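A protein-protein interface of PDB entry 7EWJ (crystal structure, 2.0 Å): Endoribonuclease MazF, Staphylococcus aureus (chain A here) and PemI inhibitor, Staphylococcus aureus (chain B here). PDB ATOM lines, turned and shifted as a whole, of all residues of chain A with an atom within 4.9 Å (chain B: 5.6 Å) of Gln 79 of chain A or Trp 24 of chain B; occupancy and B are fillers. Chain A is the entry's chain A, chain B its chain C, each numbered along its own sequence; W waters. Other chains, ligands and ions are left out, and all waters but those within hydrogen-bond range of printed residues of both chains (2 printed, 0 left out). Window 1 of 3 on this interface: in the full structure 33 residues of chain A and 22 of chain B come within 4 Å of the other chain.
Water W2 lies within hydrogen-bond range of the backbone carbonyl oxygen (O) of Leu 17 of chain A (2.7 Å), the backbone NH (N) of Glu 26 of chain B (2.8 Å) and the backbone NH (N) of Glu 25 of chain B (3.0 Å). Water W1 bridges NE1 of Trp 24 of chain B and OE1 of Gln 79 of chain A.
NH1 of Arg 81 of chain A is in hydrogen-bond range of O of Trp 24 of chain B, at 2.8 Å. O of Leu 20 of chain B lies within hydrogen-bond range of NE2 of Gln 79 of chain A (2.9 Å). O of Glu 26 of chain B sits at hydrogen-bond distance from NH1 of Arg 81 of chain A, at 2.8 Å. The side-chain amide oxygen of Gln 79 of chain A sits at hydrogen-bond distance from the backbone NH of Val 22 of chain B (2.9 Å). The side-chain hydroxyl of Tyr 17 of chain B is in hydrogen-bond range of the side-chain carboxylate of Asp 76 of chain A. NE2 of Gln 79 of chain A sits at hydrogen-bond distance from OH of Tyr 17 of chain B.
Among the printed residues, pairs that only touch across the chains: Leu 17 of chain A with Asp 23 of chain B (3.8 Å), Val 48 of chain A with Trp 24 of chain B (3.5 Å), Pro 50 of chain A with Val 22 of chain B (3.9 Å), Pro 50 of chain A with Trp 24 of chain B (3.7 Å), Val 78 of chain A with Tyr 17 of chain B (3.6 Å), Gln 79 of chain A with Glu 21 of chain B (3.3 Å), Gln 79 of chain A with Trp 24 of chain B (3.996 Å) and Ile 80 of chain A with Trp 24 of chain B (3.7 Å).
Cys 31 of chain A touches none of the printed residues of chain B. Of the printed residues of chain B, Gln 79 of chain A touches Tyr 17 (2.8 Å), Leu 20 (2.9 Å), Glu 21 (3.3 Å), Val 22 (2.9 Å) and Trp 24 (3.996 Å). Of the printed residues of chain B, Arg 81 of chain A touches Trp 24 (2.8 Å) and Glu 26 (2.8 Å). Printed residues of chain A within 4 Å of Leu 20 of chain B: Gln 79. The nearest printed residue of chain B that does not touch Gln 79 of chain A is Glu 19 of chain B (4.2 Å). The nearest printed residue of chain A that does not touch Trp 24 of chain B is Leu 49 of chain A (4.3 Å).
Hydrophobic or aromatic side chains of chain A that line the printed part of chain B: Leu 17, Val 48, Pro 50 and Val 78.
OD1 of Asp 76 of chain A lies within hydrogen-bond range of N of Val 78 of chain A, at 3.0 Å. O of Pro 50 of chain A is in hydrogen-bond range of N of Asp 76 of chain A, 3.2 Å away. O of Arg 81 of chain A is in hydrogen-bond range of N of Val 48 of chain A, at 2.9 Å.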
ATOM      1  N   LEU A  17      11.115  19.624 -17.719  1.00  0.00           N
ATOM      2  CA  LEU A  17      10.790  20.105 -19.058  1.00  0.00           C
ATOM      3  C   LEU A  17       9.751  19.231 -19.774  1.00  0.00           C
ATOM      4  O   LEU A  17       9.271  19.611 -20.861  1.00  0.00           O
ATOM      5  CB  LEU A  17      12.073  20.168 -19.916  1.00  0.00           C
ATOM      6  CG  LEU A  17      13.082  21.192 -19.342  1.00  0.00           C
ATOM      7  CD1 LEU A  17      14.357  21.147 -20.203  1.00  0.00           C
ATOM      8  CD2 LEU A  17      12.491  22.603 -19.315  1.00  0.00           C
ATOM      9  N   CYS A  31      18.646  25.026 -16.106  1.00  0.00           N
ATOM     10  CA  CYS A  31      18.287  26.187 -16.896  1.00  0.00           C
ATOM     11  C   CYS A  31      18.747  27.443 -16.175  1.00  0.00           C
ATOM     12  O   CYS A  31      18.551  27.558 -14.958  1.00  0.00           O
ATOM     13  CB  CYS A  31      16.748  26.270 -17.031  1.00  0.00           C
ATOM     14  SG  CYS A  31      15.993  24.803 -17.887  1.00  0.00           S
ATOM     15  N   VAL A  48      14.570  31.398 -19.846  1.00  0.00           N
ATOM     16  CA  VAL A  48      15.710  30.542 -19.517  1.00  0.00           C
ATOM     17  C   VAL A  48      16.539  30.278 -20.757  1.00  0.00           C
ATOM     18  O   VAL A  48      16.025  30.197 -21.889  1.00  0.00           O
ATOM     19  CB  VAL A  48      15.284  29.188 -18.878  1.00  0.00           C
ATOM     20  CG1 VAL A  48      14.796  29.407 -17.357  1.00  0.00           C
ATOM     21  CG2 VAL A  48      14.169  28.471 -19.741  1.00  0.00           C
ATOM     22  N   LEU A  49      17.852  30.137 -20.515  1.00  0.00           N
ATOM     23  CA  LEU A  49      18.777  29.579 -21.464  1.00  0.00           C
ATOM     24  C   LEU A  49      19.149  28.170 -21.017  1.00  0.00           C
ATOM     25  O   LEU A  49      19.266  27.925 -19.810  1.00  0.00           O
ATOM     26  CB  LEU A  49      20.043  30.432 -21.567  1.00  0.00           C
ATOM     27  CG  LEU A  49      19.852  31.951 -21.794  1.00  0.00           C
ATOM     28  CD1 LEU A  49      21.260  32.613 -21.835  1.00  0.00           C
ATOM     29  CD2 LEU A  49      19.114  32.160 -23.207  1.00  0.00           C
ATOM     30  N   PRO A  50      19.383  27.231 -21.953  1.00  0.00           N
ATOM     31  CA  PRO A  50      19.725  25.854 -21.544  1.00  0.00           C
ATOM     32  C   PRO A  50      21.180  25.756 -21.092  1.00  0.00           C
ATOM     33  O   PRO A  50      22.088  26.358 -21.680  1.00  0.00           O
ATOM     34  CB  PRO A  50      19.466  25.023 -22.814  1.00  0.00           C
ATOM     35  CG  PRO A  50      19.842  26.007 -23.962  1.00  0.00           C
ATOM     36  CD  PRO A  50      19.440  27.438 -23.414  1.00  0.00           C
ATOM     37  N   ASP A  76      24.084  27.768 -23.755  1.00  0.00           N
ATOM     38  CA  ASP A  76      23.859  28.062 -25.164  1.00  0.00           C
ATOM     39  C   ASP A  76      22.993  29.319 -25.232  1.00  0.00           C
ATOM     40  O   ASP A  76      21.791  29.260 -24.954  1.00  0.00           O
ATOM     41  CB  ASP A  76      23.188  26.869 -25.829  1.00  0.00           C
ATOM     42  CG  ASP A  76      23.036  27.039 -27.343  1.00  0.00           C
ATOM     43  OD1 ASP A  76      23.073  28.181 -27.839  1.00  0.00           O
ATOM     44  OD2 ASP A  76      22.885  26.015 -28.033  1.00  0.00           O
ATOM     45  N   THR A  77      23.592  30.452 -25.603  1.00  0.00           N
ATOM     46  CA  THR A  77      22.840  31.705 -25.554  1.00  0.00           C
ATOM     47  C   THR A  77      21.914  31.889 -26.755  1.00  0.00           C
ATOM     48  O   THR A  77      21.104  32.824 -26.755  1.00  0.00           O
ATOM     49  CB  THR A  77      23.787  32.922 -25.469  1.00  0.00           C
ATOM     50  OG1 THR A  77      24.606  32.991 -26.643  1.00  0.00           O
ATOM     51  CG2 THR A  77      24.715  32.840 -24.195  1.00  0.00           C
ATOM     52  N   VAL A  78      21.982  30.995 -27.740  1.00  0.00           N
ATOM     53  CA  VAL A  78      21.162  31.128 -28.950  1.00  0.00           C
ATOM     54  C   VAL A  78      19.726  30.653 -28.730  1.00  0.00           C
ATOM     55  O   VAL A  78      18.816  31.077 -29.444  1.00  0.00           O
ATOM     56  CB  VAL A  78      21.868  30.364 -30.093  1.00  0.00           C
ATOM     57  CG1 VAL A  78      20.948  30.212 -31.352  1.00  0.00           C
ATOM     58  CG2 VAL A  78      23.168  31.101 -30.478  1.00  0.00           C
ATOM     59  N   GLN A  79      19.476  29.750 -27.781  1.00  0.00           N
ATOM     60  CA  GLN A  79      18.133  29.203 -27.596  1.00  0.00           C
ATOM     61  C   GLN A  79      17.544  29.699 -26.283  1.00  0.00           C
ATOM     62  O   GLN A  79      18.198  29.648 -25.247  1.00  0.00           O
ATOM     63  CB  GLN A  79      18.157  27.666 -27.626  1.00  0.00           C
ATOM     64  CG  GLN A  79      18.682  27.198 -29.033  1.00  0.00           C
ATOM     65  CD  GLN A  79      18.357  25.744 -29.319  1.00  0.00           C
ATOM     66  OE1 GLN A  79      17.260  25.252 -28.979  1.00  0.00           O
ATOM     67  NE2 GLN A  79      19.302  25.045 -29.938  1.00  0.00           N
ATOM     68  N   ILE A  80      16.311  30.158 -26.323  1.00  0.00           N
ATOM     69  CA  ILE A  80      15.701  30.831 -25.188  1.00  0.00           C
ATOM     70  C   ILE A  80      14.265  30.367 -25.147  1.00  0.00           C
ATOM     71  O   ILE A  80      13.655  30.078 -26.183  1.00  0.00           O
ATOM     72  CB  ILE A  80      15.792  32.378 -25.275  1.00  0.00           C
ATOM     73  CG1 ILE A  80      15.231  33.016 -23.981  1.00  0.00           C
ATOM     74  CG2 ILE A  80      14.992  32.928 -26.552  1.00  0.00           C
ATOM     75  CD1 ILE A  80      15.400  34.550 -23.917  1.00  0.00           C
ATOM     76  N   ARG A  81      13.723  30.248 -23.941  1.00  0.00           N
ATOM     77  CA  ARG A  81      12.317  29.932 -23.915  1.00  0.00           C
ATOM     78  C   ARG A  81      11.707  30.550 -22.657  1.00  0.00           C
ATOM     79  O   ARG A  81      12.409  30.834 -21.688  1.00  0.00           O
ATOM     80  CB  ARG A  81      12.184  28.409 -24.029  1.00  0.00           C
ATOM     81  CG  ARG A  81      10.871  28.047 -24.379  1.00  0.00           C
ATOM     82  CD  ARG A  81      10.463  26.639 -24.767  1.00  0.00           C
ATOM     83  NE  ARG A  81       9.082  26.951 -24.426  1.00  0.00           N
ATOM     84  CZ  ARG A  81       8.160  26.102 -24.029  1.00  0.00           C
ATOM     85  NH1 ARG A  81       8.458  24.816 -23.898  1.00  0.00           N
ATOM     86  NH2 ARG A  81       7.003  26.601 -23.618  1.00  0.00           N
ATOM     87  N   TYR B  17      26.008  28.501 -36.537  1.00  0.00           N
ATOM     88  CA  TYR B  17      25.481  27.685 -35.441  1.00  0.00           C
ATOM     89  C   TYR B  17      24.577  26.616 -36.044  1.00  0.00           C
ATOM     90  O   TYR B  17      23.652  26.948 -36.789  1.00  0.00           O
ATOM     91  CB  TYR B  17      24.679  28.600 -34.505  1.00  0.00           C
ATOM     92  CG  TYR B  17      23.946  27.962 -33.360  1.00  0.00           C
ATOM     93  CD1 TYR B  17      22.653  27.508 -33.514  1.00  0.00           C
ATOM     94  CD2 TYR B  17      24.547  27.821 -32.115  1.00  0.00           C
ATOM     95  CE1 TYR B  17      21.972  26.915 -32.463  1.00  0.00           C
ATOM     96  CE2 TYR B  17      23.861  27.229 -31.054  1.00  0.00           C
ATOM     97  CZ  TYR B  17      22.578  26.794 -31.246  1.00  0.00           C
ATOM     98  OH  TYR B  17      21.852  26.246 -30.218  1.00  0.00           O
ATOM     99  N   GLU B  19      23.096  23.731 -34.196  1.00  0.00           N
ATOM    100  CA  GLU B  19      22.462  22.800 -33.266  1.00  0.00           C
ATOM    101  C   GLU B  19      20.984  22.620 -33.596  1.00  0.00           C
ATOM    102  O   GLU B  19      20.358  23.488 -34.185  1.00  0.00           O
ATOM    103  CB  GLU B  19      22.612  23.313 -31.837  1.00  0.00           C
ATOM    104  CG  GLU B  19      24.041  23.569 -31.426  1.00  0.00           C
ATOM    105  CD  GLU B  19      24.854  22.297 -31.514  1.00  0.00           C
ATOM    106  OE1 GLU B  19      24.305  21.257 -31.108  1.00  0.00           O
ATOM    107  OE2 GLU B  19      26.001  22.325 -32.034  1.00  0.00           O
ATOM    108  N   LEU B  20      20.418  21.484 -33.188  1.00  0.00           N
ATOM    109  CA  LEU B  20      18.969  21.344 -33.209  1.00  0.00           C
ATOM    110  C   LEU B  20      18.344  22.034 -31.977  1.00  0.00           C
ATOM    111  O   LEU B  20      19.037  22.356 -31.029  1.00  0.00           O
ATOM    112  CB  LEU B  20      18.587  19.860 -33.211  1.00  0.00           C
ATOM    113  CG  LEU B  20      19.191  19.076 -34.410  1.00  0.00           C
ATOM    114  CD1 LEU B  20      19.143  17.581 -34.148  1.00  0.00           C
ATOM    115  CD2 LEU B  20      18.552  19.476 -35.743  1.00  0.00           C
ATOM    116  N   GLU B  21      17.018  22.166 -31.959  1.00  0.00           N
ATOM    117  CA  GLU B  21      16.322  22.694 -30.771  1.00  0.00           C
ATOM    118  C   GLU B  21      16.660  21.826 -29.567  1.00  0.00           C
ATOM    119  O   GLU B  21      16.720  20.595 -29.680  1.00  0.00           O
ATOM    120  CB  GLU B  21      14.803  22.685 -30.975  1.00  0.00           C
ATOM    121  CG  GLU B  21      14.311  23.739 -31.991  1.00  0.00           C
ATOM    122  CD  GLU B  21      12.795  23.777 -32.159  1.00  0.00           C
ATOM    123  OE1 GLU B  21      12.097  23.027 -31.437  1.00  0.00           O
ATOM    124  OE2 GLU B  21      12.292  24.561 -33.023  1.00  0.00           O
ATOM    125  N   VAL B  22      16.906  22.457 -28.408  1.00  0.00           N
ATOM    126  CA  VAL B  22      17.157  21.670 -27.189  1.00  0.00           C
ATOM    127  C   VAL B  22      15.836  21.011 -26.797  1.00  0.00           C
ATOM    128  O   VAL B  22      14.783  21.330 -27.337  1.00  0.00           O
ATOM    129  CB  VAL B  22      17.725  22.547 -26.029  1.00  0.00           C
ATOM    130  CG1 VAL B  22      19.093  23.102 -26.443  1.00  0.00           C
ATOM    131  CG2 VAL B  22      16.776  23.705 -25.695  1.00  0.00           C
ATOM    132  N   ASP B  23      15.875  20.150 -25.802  1.00  0.00           N
ATOM    133  CA  ASP B  23      14.827  19.190 -25.458  1.00  0.00           C
ATOM    134  C   ASP B  23      13.760  19.803 -24.530  1.00  0.00           C
ATOM    135  O   ASP B  23      13.489  19.360 -23.421  1.00  0.00           O
ATOM    136  CB  ASP B  23      15.528  17.999 -24.817  1.00  0.00           C
ATOM    137  CG  ASP B  23      14.620  16.797 -24.628  1.00  0.00           C
ATOM    138  OD1 ASP B  23      13.504  16.796 -25.198  1.00  0.00           O
ATOM    139  OD2 ASP B  23      15.043  15.896 -23.858  1.00  0.00           O
ATOM    140  N   TRP B  24      13.164  20.888 -24.988  1.00  0.00           N
ATOM    141  CA  TRP B  24      12.063  21.617 -24.336  1.00  0.00           C
ATOM    142  C   TRP B  24      10.880  21.950 -25.239  1.00  0.00           C
ATOM    143  O   TRP B  24      10.266  23.014 -25.113  1.00  0.00           O
ATOM    144  CB  TRP B  24      12.375  22.937 -23.616  1.00  0.00           C
ATOM    145  CG  TRP B  24      13.163  23.787 -24.588  1.00  0.00           C
ATOM    146  CD1 TRP B  24      12.815  24.474 -25.665  1.00  0.00           C
ATOM    147  CD2 TRP B  24      13.957  24.863 -23.921  1.00  0.00           C
ATOM    148  NE1 TRP B  24      13.761  25.381 -26.060  1.00  0.00           N
ATOM    149  CE2 TRP B  24      14.366  25.789 -24.912  1.00  0.00           C
ATOM    150  CE3 TRP B  24      14.430  25.046 -22.592  1.00  0.00           C
ATOM    151  CZ2 TRP B  24      15.256  26.853 -24.660  1.00  0.00           C
ATOM    152  CZ3 TRP B  24      15.331  26.097 -22.334  1.00  0.00           C
ATOM    153  CH2 TRP B  24      15.740  26.989 -23.361  1.00  0.00           C
ATOM    154  N   GLU B  25      10.457  20.987 -26.045  1.00  0.00           N
ATOM    155  CA  GLU B  25       9.386  21.158 -27.027  1.00  0.00           C
ATOM    156  C   GLU B  25       8.007  21.324 -26.409  1.00  0.00           C
ATOM    157  O   GLU B  25       7.102  21.905 -27.042  1.00  0.00           O
ATOM    158  CB  GLU B  25       9.302  19.873 -27.876  1.00  0.00           C
ATOM    159  CG  GLU B  25      10.180  19.900 -29.010  1.00  0.00           C
ATOM    160  CD  GLU B  25       9.810  18.849 -30.034  1.00  0.00           C
ATOM    161  OE1 GLU B  25       9.953  19.213 -31.212  1.00  0.00           O
ATOM    162  OE2 GLU B  25       9.361  17.716 -29.675  1.00  0.00           O
ATOM    163  N   GLU B  26       7.757  20.663 -25.284  1.00  0.00           N
ATOM    164  CA  GLU B  26       6.385  20.599 -24.787  1.00  0.00           C
ATOM    165  C   GLU B  26       5.977  21.907 -24.128  1.00  0.00           C
ATOM    166  O   GLU B  26       6.795  22.582 -23.506  1.00  0.00           O
ATOM    167  CB  GLU B  26       6.214  19.456 -23.779  1.00  0.00           C
ATOM    168  CG  GLU B  26       6.315  18.017 -24.345  1.00  0.00           C
ATOM    169  CD  GLU B  26       5.262  17.725 -25.466  1.00  0.00           C
ATOM    170  OE1 GLU B  26       4.062  18.073 -25.292  1.00  0.00           O
ATOM    171  OE2 GLU B  26       5.625  17.114 -26.495  1.00  0.00           O
HETATM  172  O   HOH W   1      14.749  26.401 -28.432  1.00  0.00           O
HETATM  173  O   HOH W   2       9.617  19.446 -23.552  1.00  0.00           O
